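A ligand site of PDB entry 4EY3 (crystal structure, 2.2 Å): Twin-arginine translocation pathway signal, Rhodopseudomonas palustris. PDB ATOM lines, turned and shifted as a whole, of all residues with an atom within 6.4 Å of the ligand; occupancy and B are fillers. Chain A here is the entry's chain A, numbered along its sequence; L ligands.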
ATOM      1  N   GLN A  19      12.149  28.969   2.485  1.00  0.00           N
ATOM      2  CA  GLN A  19      12.754  27.696   2.105  1.00  0.00           C
ATOM      3  C   GLN A  19      13.669  27.773   0.878  1.00  0.00           C
ATOM      4  O   GLN A  19      13.959  26.752   0.251  1.00  0.00           O
ATOM      5  CB  GLN A  19      11.678  26.628   1.894  1.00  0.00           C
ATOM      6  CG  GLN A  19      10.752  26.430   3.078  1.00  0.00           C
ATOM      7  CD  GLN A  19      11.493  26.202   4.382  1.00  0.00           C
ATOM      8  OE1 GLN A  19      11.500  27.069   5.259  1.00  0.00           O
ATOM      9  NE2 GLN A  19      12.132  25.051   4.513  1.00  0.00           N
ATOM     10  N   THR A  22      16.358  25.126   0.064  1.00  0.00           N
ATOM     11  CA  THR A  22      15.904  23.863  -0.506  1.00  0.00           C
ATOM     12  C   THR A  22      15.981  23.889  -2.033  1.00  0.00           C
ATOM     13  O   THR A  22      16.628  23.030  -2.646  1.00  0.00           O
ATOM     14  CB  THR A  22      14.467  23.508  -0.048  1.00  0.00           C
ATOM     15  OG1 THR A  22      14.466  23.245   1.361  1.00  0.00           O
ATOM     16  CG2 THR A  22      13.940  22.276  -0.786  1.00  0.00           C
ATOM     17  N   GLY A  80       9.211  21.674  -2.511  1.00  0.00           N
ATOM     18  CA  GLY A  80      10.001  21.906  -1.307  1.00  0.00           C
ATOM     19  C   GLY A  80       9.326  21.589   0.007  1.00  0.00           C
ATOM     20  O   GLY A  80       9.974  21.135   0.954  1.00  0.00           O
ATOM     21  N   ILE A  81       8.020  21.832   0.077  1.00  0.00           N
ATOM     22  CA  ILE A  81       7.241  21.557   1.279  1.00  0.00           C
ATOM     23  C   ILE A  81       6.063  20.631   0.965  1.00  0.00           C
ATOM     24  O   ILE A  81       5.720  20.424  -0.207  1.00  0.00           O
ATOM     25  CB  ILE A  81       6.764  22.847   2.003  1.00  0.00           C
ATOM     26  CG1 ILE A  81       5.793  23.654   1.131  1.00  0.00           C
ATOM     27  CG2 ILE A  81       7.959  23.700   2.413  1.00  0.00           C
ATOM     28  CD1 ILE A  81       5.041  24.737   1.882  1.00  0.00           C
ATOM     29  N   THR A  82       5.457  20.056   2.009  1.00  0.00           N
ATOM     30  CA  THR A  82       4.341  19.121   1.836  1.00  0.00           C
ATOM     31  C   THR A  82       3.117  19.734   1.121  1.00  0.00           C
ATOM     32  O   THR A  82       2.620  19.145   0.162  1.00  0.00           O
ATOM     33  CB  THR A  82       3.972  18.423   3.174  1.00  0.00           C
ATOM     34  OG1 THR A  82       4.946  17.408   3.450  1.00  0.00           O
ATOM     35  CG2 THR A  82       2.585  17.792   3.125  1.00  0.00           C
ATOM     36  N   PRO A  83       2.644  20.932   1.553  1.00  0.00           N
ATOM     37  CA  PRO A  83       1.513  21.541   0.844  1.00  0.00           C
ATOM     38  C   PRO A  83       1.764  21.869  -0.637  1.00  0.00           C
ATOM     39  O   PRO A  83       0.817  21.898  -1.424  1.00  0.00           O
ATOM     40  CB  PRO A  83       1.240  22.831   1.635  1.00  0.00           C
ATOM     41  CG  PRO A  83       1.778  22.547   2.986  1.00  0.00           C
ATOM     42  CD  PRO A  83       3.009  21.720   2.752  1.00  0.00           C
ATOM     43  N   ALA A 103      11.799  16.648  -2.131  1.00  0.00           N
ATOM     44  CA  ALA A 103      12.000  17.315  -0.849  1.00  0.00           C
ATOM     45  C   ALA A 103      10.994  16.918   0.236  1.00  0.00           C
ATOM     46  O   ALA A 103      11.374  16.347   1.254  1.00  0.00           O
ATOM     47  CB  ALA A 103      12.015  18.829  -1.038  1.00  0.00           C
ATOM     48  N   ALA A 104       9.708  17.215   0.005  1.00  0.00           N
ATOM     49  CA  ALA A 104       8.649  17.004   1.005  1.00  0.00           C
ATOM     50  C   ALA A 104       8.651  15.620   1.663  1.00  0.00           C
ATOM     51  O   ALA A 104       8.834  14.604   1.001  1.00  0.00           O
ATOM     52  CB  ALA A 104       7.298  17.292   0.371  1.00  0.00           C
ATOM     53  N   GLY A 105       8.440  15.594   2.980  1.00  0.00           N
ATOM     54  CA  GLY A 105       8.599  14.347   3.754  1.00  0.00           C
ATOM     55  C   GLY A 105       7.440  13.842   4.593  1.00  0.00           C
ATOM     56  O   GLY A 105       7.649  13.105   5.561  1.00  0.00           O
ATOM     57  N   THR A 106       6.208  14.226   4.258  1.00  0.00           N
ATOM     58  CA  THR A 106       5.027  13.683   4.922  1.00  0.00           C
ATOM     59  C   THR A 106       4.658  12.327   4.313  1.00  0.00           C
ATOM     60  O   THR A 106       4.699  12.155   3.096  1.00  0.00           O
ATOM     61  CB  THR A 106       3.845  14.671   4.835  1.00  0.00           C
ATOM     62  OG1 THR A 106       4.248  15.920   5.420  1.00  0.00           O
ATOM     63  CG2 THR A 106       2.604  14.151   5.557  1.00  0.00           C
ATOM     64  N   ILE A 109       1.848  11.682   1.287  1.00  0.00           N
ATOM     65  CA  ILE A 109       2.044  12.322  -0.008  1.00  0.00           C
ATOM     66  C   ILE A 109       1.904  11.363  -1.204  1.00  0.00           C
ATOM     67  O   ILE A 109       1.207  11.675  -2.168  1.00  0.00           O
ATOM     68  CB  ILE A 109       3.381  13.100  -0.062  1.00  0.00           C
ATOM     69  CG1 ILE A 109       3.291  14.363   0.808  1.00  0.00           C
ATOM     70  CG2 ILE A 109       3.738  13.480  -1.495  1.00  0.00           C
ATOM     71  CD1 ILE A 109       4.617  15.034   1.082  1.00  0.00           C
ATOM     72  N   ARG A 118       8.703   9.495  -4.888  1.00  0.00           N
ATOM     73  CA  ARG A 118       9.515  10.296  -3.966  1.00  0.00           C
ATOM     74  C   ARG A 118      10.977   9.814  -3.901  1.00  0.00           C
ATOM     75  O   ARG A 118      11.232   8.618  -3.786  1.00  0.00           O
ATOM     76  CB  ARG A 118       8.881  10.310  -2.578  1.00  0.00           C
ATOM     77  CG  ARG A 118       9.712  10.949  -1.477  1.00  0.00           C
ATOM     78  CD  ARG A 118       8.846  11.536  -0.375  1.00  0.00           C
ATOM     79  NE  ARG A 118       7.825  10.605   0.119  1.00  0.00           N
ATOM     80  CZ  ARG A 118       6.821  10.963   0.907  1.00  0.00           C
ATOM     81  NH1 ARG A 118       6.696  12.232   1.299  1.00  0.00           N
ATOM     82  NH2 ARG A 118       5.933  10.066   1.309  1.00  0.00           N
ATOM     83  N   PHE A 121      12.557  11.453   1.364  1.00  0.00           N
ATOM     84  CA  PHE A 121      12.436  10.763   2.650  1.00  0.00           C
ATOM     85  C   PHE A 121      11.014  10.885   3.171  1.00  0.00           C
ATOM     86  O   PHE A 121      10.208  11.624   2.621  1.00  0.00           O
ATOM     87  CB  PHE A 121      13.389  11.403   3.684  1.00  0.00           C
ATOM     88  CG  PHE A 121      13.283  12.910   3.758  1.00  0.00           C
ATOM     89  CD1 PHE A 121      12.266  13.529   4.470  1.00  0.00           C
ATOM     90  CD2 PHE A 121      14.221  13.714   3.097  1.00  0.00           C
ATOM     91  CE1 PHE A 121      12.164  14.914   4.530  1.00  0.00           C
ATOM     92  CE2 PHE A 121      14.128  15.098   3.155  1.00  0.00           C
ATOM     93  CZ  PHE A 121      13.098  15.696   3.867  1.00  0.00           C
ATOM     94  N   LEU A 123       9.537  11.700   7.194  1.00  0.00           N
ATOM     95  CA  LEU A 123       9.934  11.996   8.572  1.00  0.00           C
ATOM     96  C   LEU A 123       9.816  10.787   9.496  1.00  0.00           C
ATOM     97  O   LEU A 123      10.625  10.629  10.407  1.00  0.00           O
ATOM     98  CB  LEU A 123       9.132  13.174   9.130  1.00  0.00           C
ATOM     99  CG  LEU A 123       9.814  14.543   9.071  1.00  0.00           C
ATOM    100  CD1 LEU A 123      11.127  14.519   9.849  1.00  0.00           C
ATOM    101  CD2 LEU A 123      10.038  15.005   7.637  1.00  0.00           C
ATOM    102  N   TYR A 149       3.033  21.860  11.137  1.00  0.00           N
ATOM    103  CA  TYR A 149       2.364  21.346   9.939  1.00  0.00           C
ATOM    104  C   TYR A 149       2.714  19.866   9.712  1.00  0.00           C
ATOM    105  O   TYR A 149       3.481  19.288  10.473  1.00  0.00           O
ATOM    106  CB  TYR A 149       2.607  22.233   8.692  1.00  0.00           C
ATOM    107  CG  TYR A 149       3.976  22.170   8.055  1.00  0.00           C
ATOM    108  CD1 TYR A 149       4.100  21.976   6.668  1.00  0.00           C
ATOM    109  CD2 TYR A 149       5.143  22.325   8.801  1.00  0.00           C
ATOM    110  CE1 TYR A 149       5.353  21.920   6.062  1.00  0.00           C
ATOM    111  CE2 TYR A 149       6.397  22.272   8.205  1.00  0.00           C
ATOM    112  CZ  TYR A 149       6.492  22.066   6.839  1.00  0.00           C
ATOM    113  OH  TYR A 149       7.728  22.016   6.245  1.00  0.00           O
ATOM    114  N   ALA A 150       2.152  19.289   8.654  1.00  0.00           N
ATOM    115  CA  ALA A 150       2.141  17.829   8.449  1.00  0.00           C
ATOM    116  C   ALA A 150       3.420  17.018   8.758  1.00  0.00           C
ATOM    117  O   ALA A 150       3.334  16.012   9.478  1.00  0.00           O
ATOM    118  CB  ALA A 150       1.595  17.486   7.063  1.00  0.00           C
ATOM    119  N   PRO A 151       4.599  17.440   8.232  1.00  0.00           N
ATOM    120  CA  PRO A 151       5.809  16.637   8.487  1.00  0.00           C
ATOM    121  C   PRO A 151       6.241  16.685   9.952  1.00  0.00           C
ATOM    122  O   PRO A 151       6.807  15.702  10.460  1.00  0.00           O
ATOM    123  CB  PRO A 151       6.868  17.302   7.602  1.00  0.00           C
ATOM    124  CG  PRO A 151       6.388  18.694   7.402  1.00  0.00           C
ATOM    125  CD  PRO A 151       4.891  18.592   7.357  1.00  0.00           C
ATOM    126  N   LEU A 178       5.763  27.374  10.374  1.00  0.00           N
ATOM    127  CA  LEU A 178       6.731  27.156   9.311  1.00  0.00           C
ATOM    128  C   LEU A 178       7.406  28.466   8.930  1.00  0.00           C
ATOM    129  O   LEU A 178       8.631  28.516   8.777  1.00  0.00           O
ATOM    130  CB  LEU A 178       6.036  26.540   8.089  1.00  0.00           C
ATOM    131  CG  LEU A 178       6.780  26.450   6.747  1.00  0.00           C
ATOM    132  CD1 LEU A 178       7.886  25.407   6.782  1.00  0.00           C
ATOM    133  CD2 LEU A 178       5.803  26.162   5.621  1.00  0.00           C
ATOM    134  N   PHE A 201      12.306  19.057  15.444  1.00  0.00           N
ATOM    135  CA  PHE A 201      12.160  19.081  13.994  1.00  0.00           C
ATOM    136  C   PHE A 201      11.888  20.488  13.479  1.00  0.00           C
ATOM    137  O   PHE A 201      10.902  21.127  13.857  1.00  0.00           O
ATOM    138  CB  PHE A 201      11.068  18.137  13.465  1.00  0.00           C
ATOM    139  CG  PHE A 201      10.716  18.398  12.020  1.00  0.00           C
ATOM    140  CD1 PHE A 201      11.564  17.978  10.994  1.00  0.00           C
ATOM    141  CD2 PHE A 201       9.563  19.114  11.675  1.00  0.00           C
ATOM    142  CE1 PHE A 201      11.262  18.245   9.666  1.00  0.00           C
ATOM    143  CE2 PHE A 201       9.261  19.372  10.350  1.00  0.00           C
ATOM    144  CZ  PHE A 201      10.099  18.936   9.342  1.00  0.00           C
ATOM    145  N   VAL A 202      12.757  20.940  12.586  1.00  0.00           N
ATOM    146  CA  VAL A 202      12.527  22.131  11.791  1.00  0.00           C
ATOM    147  C   VAL A 202      12.974  21.797  10.366  1.00  0.00           C
ATOM    148  O   VAL A 202      13.987  21.111  10.191  1.00  0.00           O
ATOM    149  CB  VAL A 202      13.262  23.374  12.355  1.00  0.00           C
ATOM    150  CG1 VAL A 202      12.564  23.886  13.610  1.00  0.00           C
ATOM    151  CG2 VAL A 202      14.729  23.073  12.637  1.00  0.00           C
ATOM    152  N   PRO A 203      12.225  22.264   9.348  1.00  0.00           N
ATOM    153  CA  PRO A 203      12.547  21.948   7.952  1.00  0.00           C
ATOM    154  C   PRO A 203      13.929  22.445   7.554  1.00  0.00           C
ATOM    155  O   PRO A 203      14.445  23.392   8.175  1.00  0.00           O
ATOM    156  CB  PRO A 203      11.473  22.718   7.166  1.00  0.00           C
ATOM    157  CG  PRO A 203      11.054  23.822   8.070  1.00  0.00           C
ATOM    158  CD  PRO A 203      11.087  23.205   9.441  1.00  0.00           C
ATOM    159  N   ALA A 204      14.520  21.812   6.544  1.00  0.00           N
ATOM    160  CA  ALA A 204      15.788  22.267   5.978  1.00  0.00           C
ATOM    161  C   ALA A 204      15.819  23.781   5.882  1.00  0.00           C
ATOM    162  O   ALA A 204      14.808  24.404   5.541  1.00  0.00           O
ATOM    163  CB  ALA A 204      16.007  21.649   4.607  1.00  0.00           C
ATOM    164  N   GLY A 205      16.960  24.375   6.208  1.00  0.00           N
ATOM    165  CA  GLY A 205      17.136  25.817   6.117  1.00  0.00           C
ATOM    166  C   GLY A 205      16.921  26.577   7.408  1.00  0.00           C
ATOM    167  O   GLY A 205      17.197  27.776   7.487  1.00  0.00           O
ATOM    168  N   ASP A 231      17.037  16.928   9.907  1.00  0.00           N
ATOM    169  CA  ASP A 231      16.672  18.211   9.290  1.00  0.00           C
ATOM    170  C   ASP A 231      17.292  19.437   9.969  1.00  0.00           C
ATOM    171  O   ASP A 231      17.811  20.337   9.295  1.00  0.00           O
ATOM    172  CB  ASP A 231      15.146  18.359   9.200  1.00  0.00           C
ATOM    173  CG  ASP A 231      14.481  17.161   8.532  1.00  0.00           C
ATOM    174  OD1 ASP A 231      14.028  17.295   7.375  1.00  0.00           O
ATOM    175  OD2 ASP A 231      14.443  16.077   9.161  1.00  0.00           O
ATOM    176  N   HIS A 252      19.058  10.199  10.166  1.00  0.00           N
ATOM    177  CA  HIS A 252      18.799  10.747   8.832  1.00  0.00           C
ATOM    178  C   HIS A 252      19.293   9.872   7.718  1.00  0.00           C
ATOM    179  O   HIS A 252      20.077   8.949   7.948  1.00  0.00           O
ATOM    180  CB  HIS A 252      19.411  12.139   8.704  1.00  0.00           C
ATOM    181  CG  HIS A 252      18.558  13.122   7.931  1.00  0.00           C
ATOM    182  ND1 HIS A 252      17.226  13.214   8.079  1.00  0.00           N
ATOM    183  CD2 HIS A 252      18.912  14.090   6.999  1.00  0.00           C
ATOM    184  CE1 HIS A 252      16.744  14.176   7.282  1.00  0.00           C
ATOM    185  NE2 HIS A 252      17.783  14.717   6.616  1.00  0.00           N
ATOM    186  N   PHE A 280      21.104  17.479   2.442  1.00  0.00           N
ATOM    187  CA  PHE A 280      20.217  16.359   2.114  1.00  0.00           C
ATOM    188  C   PHE A 280      19.150  16.693   1.054  1.00  0.00           C
ATOM    189  O   PHE A 280      18.633  15.802   0.382  1.00  0.00           O
ATOM    190  CB  PHE A 280      19.582  15.757   3.376  1.00  0.00           C
ATOM    191  CG  PHE A 280      18.642  16.679   4.090  1.00  0.00           C
ATOM    192  CD1 PHE A 280      17.271  16.651   3.824  1.00  0.00           C
ATOM    193  CD2 PHE A 280      19.104  17.553   5.068  1.00  0.00           C
ATOM    194  CE1 PHE A 280      16.405  17.488   4.488  1.00  0.00           C
ATOM    195  CE2 PHE A 280      18.231  18.404   5.739  1.00  0.00           C
ATOM    196  CZ  PHE A 280      16.875  18.358   5.455  1.00  0.00           C
ATOM    197  N   MET A 281      18.829  17.976   0.902  1.00  0.00           N
ATOM    198  CA  MET A 281      17.927  18.424  -0.165  1.00  0.00           C
ATOM    199  C   MET A 281      18.555  18.265  -1.546  1.00  0.00           C
ATOM    200  O   MET A 281      17.885  17.829  -2.490  1.00  0.00           O
ATOM    201  CB  MET A 281      17.461  19.860   0.068  1.00  0.00           C
ATOM    202  CG  MET A 281      16.431  20.014   1.176  1.00  0.00           C
ATOM    203  SD  MET A 281      15.030  18.636   1.080  1.00  0.00           S
ATOM    204  CE  MET A 281      13.776  19.448   2.333  1.00  0.00           C
HETATM  205  C1  LIG L   1       7.988  19.045   4.250  1.00  0.00           C
HETATM  206  O1  LIG L   1       7.434  17.956   4.007  1.00  0.00           O
HETATM  207  O2  LIG L   1       7.352  20.116   4.135  1.00  0.00           O
HETATM  208  C2  LIG L   1       9.419  19.088   4.692  1.00  0.00           C
HETATM  209  C3  LIG L   1      10.219  20.158   4.314  1.00  0.00           C
HETATM  210  C4  LIG L   1      11.546  20.220   4.728  1.00  0.00           C
HETATM  211  C5  LIG L   1      12.072  19.201   5.523  1.00  0.00           C
HETATM  212  C6  LIG L   1      11.272  18.122   5.905  1.00  0.00           C
HETATM  213  C7  LIG L   1       9.936  18.072   5.490  1.00  0.00           C
HETATM  214  O3  LIG L   1      13.386  19.258   5.920  1.00  0.00           O
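O1 of the ligand lies within hydrogen-bond range of N of Gly 105 (2.8 Å). An oxygen (O1) of the ligand is in hydrogen-bond range of the side-chain hydroxyl of Thr 82 (2.6 Å). O3 of the ligand sits at hydrogen-bond distance from OD1 of Asp 231 (2.5 Å). The side-chain hydroxyl (OH) of Tyr 149 is in hydrogen-bond range of an oxygen (O2) of the ligand. The backbone NH (N) of Thr 82 lies within hydrogen-bond range of an oxygen (O2) of the ligand, 2.8 Å away. N of Ala 204 is in hydrogen-bond range of O3 of the ligand, 2.9 Å away.
The side-chain hydroxyl of Thr 106 lies within hydrogen-bond range of the side-chain hydroxyl of Thr 82, at 2.6 Å. O of Ala 204 lies within hydrogen-bond range of NE2 of Gln 19. O of Ala 104 is in hydrogen-bond range of NH1 of Arg 118 (3.2 Å). N of Leu 123 is in hydrogen-bond range of O of Gly 105, at 2.9 Å. O of Thr 106 is in hydrogen-bond range of NH1 of Arg 118, 2.7 Å away.
O of Gly 80 touches C3 of the ligand, at 3.5 Å. Ile 81 touches the ligand. CA of Ala 104 touches O1 of the ligand, 3.4 Å away. Thr 106 touches the ligand. CE1 of Phe 121 touches C6 of the ligand, 3.6 Å away. Leu 123 touches the ligand (CD2 to C7, 3.7 Å). CG of Pro 151 touches C1 of the ligand (3.6 Å). Phe 201 touches the ligand (CZ to C6, 3.7 Å). Pro 203 touches the ligand (CA to O3, 3.5 Å). Phe 280 touches the ligand. Met 281 touches the ligand. Hydrophobic or aromatic side chains that line the ligand: Ile 81, Ala 104, Phe 121, Leu 123, Tyr 149, Pro 151, Phe 201, Pro 203, Ala 204, Phe 280 and Met 281. Within 4 Å of the ligand: Gly 80, Ile 81, Thr 82, Ala 104, Gly 105, Thr 106, Phe 121, Leu 123, Tyr 149, Pro 151, Phe 201, Pro 203, Ala 204, Asp 231, Phe 280 and Met 281. Along chain A the residues within 4 Å of the ligand span positions 80 to 281.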
